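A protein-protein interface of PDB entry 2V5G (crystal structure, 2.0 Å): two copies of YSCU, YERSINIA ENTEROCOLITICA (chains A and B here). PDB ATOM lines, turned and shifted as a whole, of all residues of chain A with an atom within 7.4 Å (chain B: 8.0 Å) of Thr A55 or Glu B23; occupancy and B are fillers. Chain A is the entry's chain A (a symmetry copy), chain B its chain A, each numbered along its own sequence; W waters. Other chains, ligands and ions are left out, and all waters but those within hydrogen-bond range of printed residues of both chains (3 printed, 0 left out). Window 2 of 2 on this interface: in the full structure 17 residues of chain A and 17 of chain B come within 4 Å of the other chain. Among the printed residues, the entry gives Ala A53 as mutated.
NE of Arg B29 is in salt-bridge range of OD1 of Asp A79, at 2.7 Å.
NH2 of Arg B29 sits at hydrogen-bond distance from O of Thr A55, at 3.0 Å.
The side-chain amide oxygen of Gln B30 lies within hydrogen-bond range of the backbone NH of Gln A81, at 3.5 Å.
NH2 of Arg B29 sits close to ND1 of His A56, at 3.4 Å.
NE of Arg B29 is in hydrogen-bond range of O of Trp B108 (3.0 Å).
The backbone carbonyl oxygen (O) of Asp A79 lies within hydrogen-bond range of the side-chain amide nitrogen (NE2) of Gln A83.
N of Glu B23 lies close to OG of Ser B21, at 3.3 Å.
The backbone NH of Thr A55 sits at hydrogen-bond distance from the side-chain amide oxygen of Gln A83 (3.5 Å).
The side-chain hydroxyl (OG) of Ser B26 sits at hydrogen-bond distance from the backbone carbonyl oxygen (O) of Glu B23, at 2.8 Å.
The backbone NH of Asp A79 sits at hydrogen-bond distance from the backbone carbonyl oxygen of His A56, 3.0 Å away.
Among the printed residues, merely in contact across the chains: Ala A80 with Gln B30 (3.2 Å), Thr A55 with Ser B26 (3.4 Å), Ile A57 with Trp B108 (3.5 Å), His A56 with Trp B108 (3.5 Å), Ala A80 with Ser B26 (3.5 Å), Gln A83 with Ser B26 (3.6 Å), Asp A79 with Ser B26 (3.6 Å), Ala A80 with Lys B27 (3.6 Å), His A56 with Asp B109 (3.7 Å), Thr A55 with Glu B23 (3.7 Å) and Thr A55 with Pro B22 (3.8 Å).
Water W3 lies within hydrogen-bond range of ND1 of His A56 (2.5 Å), O of Trp B108 (2.7 Å), OD1 of Asp A79 (2.7 Å) and NE of Arg B29 (3.2 Å).
Water W1 lies within hydrogen-bond range of the backbone carbonyl oxygen of Pro B22 (2.7 Å), the side-chain hydroxyl of Thr A55 (2.8 Å) and the guanidinium group of Arg B29 (3.0 Å).
Water W2 lies within hydrogen-bond range of the side-chain amide oxygen (OE1) of Gln B30 (2.7 Å) and the backbone NH (N) of Gln A81 (3.4 Å).
Pro A54 touches none of the printed residues of chain B.
Of chain B, only Pro B22 (3.8 Å), Glu B23 (3.7 Å), Ser B26 (3.4 Å) and Arg B29 (3.0 Å) come within 4 Å of Thr A55.
Printed residues of chain B within 4 Å of Ile A57: Trp B108.
Printed residues of chain B within 4 Å of Gln A83: Ser B26 (3.6 Å).
Of chain A, only Thr A55 (3.7 Å) comes within 4 Å of Glu B23.
Ile B24 touches none of the printed residues of chain A.
Of the printed residues of chain A, Ser B26 touches Thr A55, Asp A79, Ala A80 and Gln A83.
Printed residues of chain A within 4 Å of Trp B108: His A56 (3.5 Å) and Ile A57 (3.5 Å).
Along chain B the printed residues that touch a printed residue of chain A span positions 22 to 109.
Of the 14 printed residues of chain A, 7 touch a printed residue of chain B.
No position is printed for both chains.
Of the 15 pairs that touch across the chains among the printed residues, none has its exchanged pair printed and touching as well.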
ATOM      1  N   ALA A  52       6.684 -37.544  13.300  1.00  0.00           N
ATOM      2  CA  ALA A  52       6.716 -36.150  13.703  1.00  0.00           C
ATOM      3  C   ALA A  52       8.088 -35.612  14.052  1.00  0.00           C
ATOM      4  O   ALA A  52       8.980 -36.375  14.430  1.00  0.00           O
ATOM      5  CB  ALA A  52       5.739 -35.937  14.915  1.00  0.00           C
ATOM      6  N   ALA A  53       8.245 -34.300  13.844  1.00  0.00           N
ATOM      7  CA  ALA A  53       9.281 -33.475  14.432  1.00  0.00           C
ATOM      8  C   ALA A  53       8.486 -32.513  15.361  1.00  0.00           C
ATOM      9  O   ALA A  53       7.871 -31.534  14.880  1.00  0.00           O
ATOM     10  CB  ALA A  53      10.058 -32.708  13.367  1.00  0.00           C
ATOM     11  N   PRO A  54       8.432 -32.816  16.689  1.00  0.00           N
ATOM     12  CA  PRO A  54       7.591 -32.048  17.643  1.00  0.00           C
ATOM     13  C   PRO A  54       7.689 -30.523  17.435  1.00  0.00           C
ATOM     14  O   PRO A  54       8.781 -29.992  17.231  1.00  0.00           O
ATOM     15  CB  PRO A  54       8.153 -32.433  19.013  1.00  0.00           C
ATOM     16  CG  PRO A  54       8.854 -33.747  18.802  1.00  0.00           C
ATOM     17  CD  PRO A  54       9.228 -33.875  17.360  1.00  0.00           C
ATOM     18  N   THR A  55       6.532 -29.876  17.412  1.00  0.00           N
ATOM     19  CA  THR A  55       6.321 -28.414  17.187  1.00  0.00           C
ATOM     20  C   THR A  55       6.693 -27.921  15.802  1.00  0.00           C
ATOM     21  O   THR A  55       6.607 -26.712  15.520  1.00  0.00           O
ATOM     22  CB  THR A  55       6.961 -27.494  18.276  1.00  0.00           C
ATOM     23  OG1 THR A  55       8.367 -27.398  18.071  1.00  0.00           O
ATOM     24  CG2 THR A  55       6.647 -28.016  19.708  1.00  0.00           C
ATOM     25  N   HIS A  56       7.069 -28.847  14.917  1.00  0.00           N
ATOM     26  CA  HIS A  56       7.452 -28.467  13.551  1.00  0.00           C
ATOM     27  C   HIS A  56       6.673 -29.207  12.449  1.00  0.00           C
ATOM     28  O   HIS A  56       6.083 -28.565  11.573  1.00  0.00           O
ATOM     29  CB  HIS A  56       8.976 -28.612  13.378  1.00  0.00           C
ATOM     30  CG  HIS A  56       9.777 -27.625  14.188  1.00  0.00           C
ATOM     31  ND1 HIS A  56       9.849 -26.278  13.873  1.00  0.00           N
ATOM     32  CD2 HIS A  56      10.517 -27.784  15.307  1.00  0.00           C
ATOM     33  CE1 HIS A  56      10.601 -25.659  14.765  1.00  0.00           C
ATOM     34  NE2 HIS A  56      11.018 -26.547  15.647  1.00  0.00           N
ATOM     35  N   ILE A  57       6.645 -30.538  12.487  1.00  0.00           N
ATOM     36  CA  ILE A  57       6.117 -31.347  11.350  1.00  0.00           C
ATOM     37  C   ILE A  57       5.342 -32.562  11.843  1.00  0.00           C
ATOM     38  O   ILE A  57       5.797 -33.236  12.765  1.00  0.00           O
ATOM     39  CB  ILE A  57       7.299 -31.943  10.502  1.00  0.00           C
ATOM     40  CG1 ILE A  57       8.287 -30.865  10.073  1.00  0.00           C
ATOM     41  CG2 ILE A  57       6.769 -32.764   9.286  1.00  0.00           C
ATOM     42  CD1 ILE A  57       9.556 -31.398   9.399  1.00  0.00           C
ATOM     43  N   ALA A  58       4.177 -32.822  11.247  1.00  0.00           N
ATOM     44  CA  ALA A  58       3.499 -34.101  11.411  1.00  0.00           C
ATOM     45  C   ALA A  58       3.180 -34.606  10.010  1.00  0.00           C
ATOM     46  O   ALA A  58       2.598 -33.867   9.219  1.00  0.00           O
ATOM     47  CB  ALA A  58       2.212 -33.942  12.222  1.00  0.00           C
ATOM     48  N   THR A  78       2.004 -28.543  10.032  1.00  0.00           N
ATOM     49  CA  THR A  78       3.197 -27.881  10.547  1.00  0.00           C
ATOM     50  C   THR A  78       2.885 -26.976  11.724  1.00  0.00           C
ATOM     51  O   THR A  78       1.733 -26.538  11.909  1.00  0.00           O
ATOM     52  CB  THR A  78       3.894 -26.995   9.476  1.00  0.00           C
ATOM     53  OG1 THR A  78       3.006 -25.961   9.072  1.00  0.00           O
ATOM     54  CG2 THR A  78       4.288 -27.806   8.238  1.00  0.00           C
ATOM     55  N   ASP A  79       3.929 -26.689  12.495  1.00  0.00           N
ATOM     56  CA  ASP A  79       3.842 -25.752  13.595  1.00  0.00           C
ATOM     57  C   ASP A  79       2.767 -26.172  14.600  1.00  0.00           C
ATOM     58  O   ASP A  79       2.737 -27.337  15.012  1.00  0.00           O
ATOM     59  CB  ASP A  79       3.690 -24.299  13.060  1.00  0.00           C
ATOM     60  CG  ASP A  79       4.981 -23.759  12.466  1.00  0.00           C
ATOM     61  OD1 ASP A  79       6.098 -24.100  12.958  1.00  0.00           O
ATOM     62  OD2 ASP A  79       4.883 -22.968  11.519  1.00  0.00           O
ATOM     63  N   ALA A  80       1.898 -25.249  15.016  1.00  0.00           N
ATOM     64  CA  ALA A  80       0.923 -25.530  16.093  1.00  0.00           C
ATOM     65  C   ALA A  80      -0.084 -26.625  15.748  1.00  0.00           C
ATOM     66  O   ALA A  80      -0.666 -27.247  16.648  1.00  0.00           O
ATOM     67  CB  ALA A  80       0.183 -24.237  16.534  1.00  0.00           C
ATOM     68  N   GLN A  81      -0.299 -26.843  14.452  1.00  0.00           N
ATOM     69  CA  GLN A  81      -1.174 -27.925  13.978  1.00  0.00           C
ATOM     70  C   GLN A  81      -0.725 -29.308  14.454  1.00  0.00           C
ATOM     71  O   GLN A  81      -1.558 -30.202  14.657  1.00  0.00           O
ATOM     72  CB  GLN A  81      -1.239 -27.937  12.451  1.00  0.00           C
ATOM     73  CG  GLN A  81      -1.854 -26.728  11.821  1.00  0.00           C
ATOM     74  CD  GLN A  81      -1.739 -26.759  10.290  1.00  0.00           C
ATOM     75  OE1 GLN A  81      -0.787 -27.318   9.725  1.00  0.00           O
ATOM     76  NE2 GLN A  81      -2.699 -26.154   9.625  1.00  0.00           N
ATOM     77  N   VAL A  82       0.588 -29.464  14.658  1.00  0.00           N
ATOM     78  CA  VAL A  82       1.178 -30.725  15.097  1.00  0.00           C
ATOM     79  C   VAL A  82       0.631 -31.090  16.481  1.00  0.00           C
ATOM     80  O   VAL A  82       0.399 -32.261  16.785  1.00  0.00           O
ATOM     81  CB  VAL A  82       2.724 -30.646  15.134  1.00  0.00           C
ATOM     82  CG1 VAL A  82       3.347 -31.937  15.684  1.00  0.00           C
ATOM     83  CG2 VAL A  82       3.284 -30.330  13.744  1.00  0.00           C
ATOM     84  N   GLN A  83       0.407 -30.074  17.308  1.00  0.00           N
ATOM     85  CA  GLN A  83      -0.135 -30.299  18.641  1.00  0.00           C
ATOM     86  C   GLN A  83      -1.583 -30.804  18.558  1.00  0.00           C
ATOM     87  O   GLN A  83      -1.915 -31.768  19.238  1.00  0.00           O
ATOM     88  CB  GLN A  83       0.085 -29.053  19.516  1.00  0.00           C
ATOM     89  CG  GLN A  83       1.548 -28.954  20.091  1.00  0.00           C
ATOM     90  CD  GLN A  83       2.728 -29.105  19.061  1.00  0.00           C
ATOM     91  OE1 GLN A  83       3.435 -30.165  19.006  1.00  0.00           O
ATOM     92  NE2 GLN A  83       2.966 -28.030  18.277  1.00  0.00           N
ATOM     93  N   ARG A  86      -1.501 -34.484  17.359  1.00  0.00           N
ATOM     94  CA  ARG A  86      -1.120 -35.310  18.507  1.00  0.00           C
ATOM     95  C   ARG A  86      -2.319 -35.651  19.404  1.00  0.00           C
ATOM     96  O   ARG A  86      -2.528 -36.822  19.783  1.00  0.00           O
ATOM     97  CB  ARG A  86      -0.034 -34.597  19.322  1.00  0.00           C
ATOM     98  CG  ARG A  86       1.363 -34.716  18.758  1.00  0.00           C
ATOM     99  CD  ARG A  86       2.430 -34.075  19.672  1.00  0.00           C
ATOM    100  NE  ARG A  86       3.540 -35.014  19.924  1.00  0.00           N
ATOM    101  CZ  ARG A  86       4.629 -35.185  19.156  1.00  0.00           C
ATOM    102  NH1 ARG A  86       4.810 -34.453  18.052  1.00  0.00           N
ATOM    103  NH2 ARG A  86       5.557 -36.102  19.488  1.00  0.00           N
ATOM    104  N   GLY B  20       8.939 -18.244  26.520  1.00  0.00           N
ATOM    105  CA  GLY B  20       8.034 -19.324  26.132  1.00  0.00           C
ATOM    106  C   GLY B  20       8.590 -20.635  25.598  1.00  0.00           C
ATOM    107  O   GLY B  20       9.726 -20.722  25.126  1.00  0.00           O
ATOM    108  N   SER B  21       7.747 -21.660  25.662  1.00  0.00           N
ATOM    109  CA  SER B  21       8.072 -23.000  25.228  1.00  0.00           C
ATOM    110  C   SER B  21       8.246 -23.084  23.690  1.00  0.00           C
ATOM    111  O   SER B  21       7.879 -22.142  22.974  1.00  0.00           O
ATOM    112  CB  SER B  21       6.928 -23.902  25.665  1.00  0.00           C
ATOM    113  OG  SER B  21       5.718 -23.476  25.050  1.00  0.00           O
ATOM    114  N   PRO B  22       8.817 -24.203  23.179  1.00  0.00           N
ATOM    115  CA  PRO B  22       8.752 -24.414  21.729  1.00  0.00           C
ATOM    116  C   PRO B  22       7.299 -24.451  21.218  1.00  0.00           C
ATOM    117  O   PRO B  22       7.061 -24.167  20.044  1.00  0.00           O
ATOM    118  CB  PRO B  22       9.411 -25.785  21.540  1.00  0.00           C
ATOM    119  CG  PRO B  22      10.324 -25.929  22.718  1.00  0.00           C
ATOM    120  CD  PRO B  22       9.591 -25.272  23.848  1.00  0.00           C
ATOM    121  N   GLU B  23       6.349 -24.775  22.103  1.00  0.00           N
ATOM    122  CA  GLU B  23       4.940 -24.824  21.732  1.00  0.00           C
ATOM    123  C   GLU B  23       4.391 -23.444  21.405  1.00  0.00           C
ATOM    124  O   GLU B  23       3.761 -23.265  20.362  1.00  0.00           O
ATOM    125  CB  GLU B  23       4.088 -25.511  22.805  1.00  0.00           C
ATOM    126  CG  GLU B  23       4.237 -27.035  22.856  1.00  0.00           C
ATOM    127  CD  GLU B  23       5.556 -27.531  23.496  1.00  0.00           C
ATOM    128  OE1 GLU B  23       6.288 -26.758  24.199  1.00  0.00           O
ATOM    129  OE2 GLU B  23       5.850 -28.733  23.289  1.00  0.00           O
ATOM    130  N   ILE B  24       4.657 -22.454  22.257  1.00  0.00           N
ATOM    131  CA  ILE B  24       4.137 -21.104  21.993  1.00  0.00           C
ATOM    132  C   ILE B  24       4.820 -20.519  20.772  1.00  0.00           C
ATOM    133  O   ILE B  24       4.165 -19.840  19.971  1.00  0.00           O
ATOM    134  CB  ILE B  24       4.188 -20.154  23.216  1.00  0.00           C
ATOM    135  CG1 ILE B  24       3.566 -18.808  22.853  1.00  0.00           C
ATOM    136  CG2 ILE B  24       5.608 -19.945  23.689  1.00  0.00           C
ATOM    137  CD1 ILE B  24       3.235 -17.935  24.060  1.00  0.00           C
ATOM    138  N   LYS B  25       6.122 -20.805  20.614  1.00  0.00           N
ATOM    139  CA  LYS B  25       6.846 -20.338  19.433  1.00  0.00           C
ATOM    140  C   LYS B  25       6.200 -20.884  18.157  1.00  0.00           C
ATOM    141  O   LYS B  25       6.105 -20.156  17.177  1.00  0.00           O
ATOM    142  CB  LYS B  25       8.357 -20.638  19.498  1.00  0.00           C
ATOM    143  CG  LYS B  25       9.026 -20.132  20.803  1.00  0.00           C
ATOM    144  CD  LYS B  25      10.524 -19.808  20.679  1.00  0.00           C
ATOM    145  CE  LYS B  25      10.770 -18.374  20.219  1.00  0.00           C
ATOM    146  NZ  LYS B  25      10.517 -18.208  18.760  1.00  0.00           N
ATOM    147  N   SER B  26       5.728 -22.138  18.177  1.00  0.00           N
ATOM    148  CA  SER B  26       5.055 -22.681  16.976  1.00  0.00           C
ATOM    149  C   SER B  26       3.693 -22.003  16.740  1.00  0.00           C
ATOM    150  O   SER B  26       3.282 -21.794  15.597  1.00  0.00           O
ATOM    151  CB  SER B  26       4.937 -24.204  17.010  1.00  0.00           C
ATOM    152  OG  SER B  26       3.886 -24.609  17.863  1.00  0.00           O
ATOM    153  N   LYS B  27       2.988 -21.668  17.818  1.00  0.00           N
ATOM    154  CA  LYS B  27       1.716 -20.950  17.678  1.00  0.00           C
ATOM    155  C   LYS B  27       1.992 -19.540  17.130  1.00  0.00           C
ATOM    156  O   LYS B  27       1.270 -19.075  16.251  1.00  0.00           O
ATOM    157  CB  LYS B  27       0.973 -20.879  19.007  1.00  0.00           C
ATOM    158  CG  LYS B  27       0.553 -22.276  19.558  1.00  0.00           C
ATOM    159  CD  LYS B  27      -0.062 -22.246  20.971  1.00  0.00           C
ATOM    160  CE  LYS B  27      -1.390 -21.515  21.002  1.00  0.00           C
ATOM    161  NZ  LYS B  27      -2.034 -21.691  22.344  1.00  0.00           N
ATOM    162  N   ARG B  28       3.041 -18.879  17.636  1.00  0.00           N
ATOM    163  CA  ARG B  28       3.432 -17.551  17.108  1.00  0.00           C
ATOM    164  C   ARG B  28       3.807 -17.581  15.649  1.00  0.00           C
ATOM    165  O   ARG B  28       3.455 -16.642  14.919  1.00  0.00           O
ATOM    166  CB  ARG B  28       4.598 -16.933  17.892  1.00  0.00           C
ATOM    167  CG  ARG B  28       4.241 -16.517  19.298  1.00  0.00           C
ATOM    168  CD  ARG B  28       5.499 -16.068  20.039  1.00  0.00           C
ATOM    169  NE  ARG B  28       5.916 -14.714  19.649  1.00  0.00           N
ATOM    170  CZ  ARG B  28       7.158 -14.231  19.799  1.00  0.00           C
ATOM    171  NH1 ARG B  28       8.134 -14.978  20.310  1.00  0.00           N
ATOM    172  NH2 ARG B  28       7.438 -12.994  19.407  1.00  0.00           N
ATOM    173  N   ARG B  29       4.557 -18.620  15.236  1.00  0.00           N
ATOM    174  CA  ARG B  29       4.955 -18.776  13.840  1.00  0.00           C
ATOM    175  C   ARG B  29       3.732 -18.913  12.950  1.00  0.00           C
ATOM    176  O   ARG B  29       3.625 -18.234  11.935  1.00  0.00           O
ATOM    177  CB  ARG B  29       5.862 -20.018  13.643  1.00  0.00           C
ATOM    178  CG  ARG B  29       7.341 -19.757  13.810  1.00  0.00           C
ATOM    179  CD  ARG B  29       8.247 -20.899  13.274  1.00  0.00           C
ATOM    180  NE  ARG B  29       7.867 -22.214  13.788  1.00  0.00           N
ATOM    181  CZ  ARG B  29       8.248 -22.765  14.946  1.00  0.00           C
ATOM    182  NH1 ARG B  29       9.100 -22.177  15.757  1.00  0.00           N
ATOM    183  NH2 ARG B  29       7.795 -23.967  15.256  1.00  0.00           N
ATOM    184  N   GLN B  30       2.809 -19.801  13.339  1.00  0.00           N
ATOM    185  CA  GLN B  30       1.592 -20.039  12.579  1.00  0.00           C
ATOM    186  C   GLN B  30       0.738 -18.777  12.499  1.00  0.00           C
ATOM    187  O   GLN B  30       0.299 -18.365  11.393  1.00  0.00           O
ATOM    188  CB  GLN B  30       0.775 -21.203  13.163  1.00  0.00           C
ATOM    189  CG  GLN B  30      -0.407 -21.571  12.243  1.00  0.00           C
ATOM    190  CD  GLN B  30      -1.282 -22.675  12.788  1.00  0.00           C
ATOM    191  OE1 GLN B  30      -0.842 -23.510  13.566  1.00  0.00           O
ATOM    192  NE2 GLN B  30      -2.524 -22.705  12.338  1.00  0.00           N
ATOM    193  N   TRP B 108      11.964 -23.152   9.256  1.00  0.00           N
ATOM    194  CA  TRP B 108      11.519 -23.801  10.474  1.00  0.00           C
ATOM    195  C   TRP B 108      11.433 -22.898  11.695  1.00  0.00           C
ATOM    196  O   TRP B 108      10.475 -23.035  12.486  1.00  0.00           O
ATOM    197  CB  TRP B 108      12.399 -25.031  10.788  1.00  0.00           C
ATOM    198  CG  TRP B 108      12.268 -26.136   9.759  1.00  0.00           C
ATOM    199  CD1 TRP B 108      13.273 -26.702   9.049  1.00  0.00           C
ATOM    200  CD2 TRP B 108      11.049 -26.753   9.289  1.00  0.00           C
ATOM    201  NE1 TRP B 108      12.767 -27.646   8.178  1.00  0.00           N
ATOM    202  CE2 TRP B 108      11.406 -27.676   8.291  1.00  0.00           C
ATOM    203  CE3 TRP B 108       9.697 -26.598   9.609  1.00  0.00           C
ATOM    204  CZ2 TRP B 108      10.452 -28.473   7.610  1.00  0.00           C
ATOM    205  CZ3 TRP B 108       8.734 -27.379   8.926  1.00  0.00           C
ATOM    206  CH2 TRP B 108       9.125 -28.285   7.927  1.00  0.00           C
ATOM    207  N   ASP B 109      12.406 -21.985  11.851  1.00  0.00           N
ATOM    208  CA  ASP B 109      12.539 -21.270  13.103  1.00  0.00           C
ATOM    209  C   ASP B 109      12.111 -19.822  13.113  1.00  0.00           C
ATOM    210  O   ASP B 109      11.739 -19.312  14.178  1.00  0.00           O
ATOM    211  CB  ASP B 109      13.996 -21.345  13.604  1.00  0.00           C
ATOM    212  CG  ASP B 109      14.474 -22.779  13.829  1.00  0.00           C
ATOM    213  OD1 ASP B 109      13.659 -23.650  14.205  1.00  0.00           O
ATOM    214  OD2 ASP B 109      15.677 -23.029  13.599  1.00  0.00           O
HETATM  215  O   HOH W   1       8.831 -24.624  18.031  1.00  0.00           O
HETATM  216  O   HOH W   2      -2.979 -24.754  14.736  1.00  0.00           O
HETATM  217  O   HOH W   3       8.569 -24.895  12.219  1.00  0.00           O
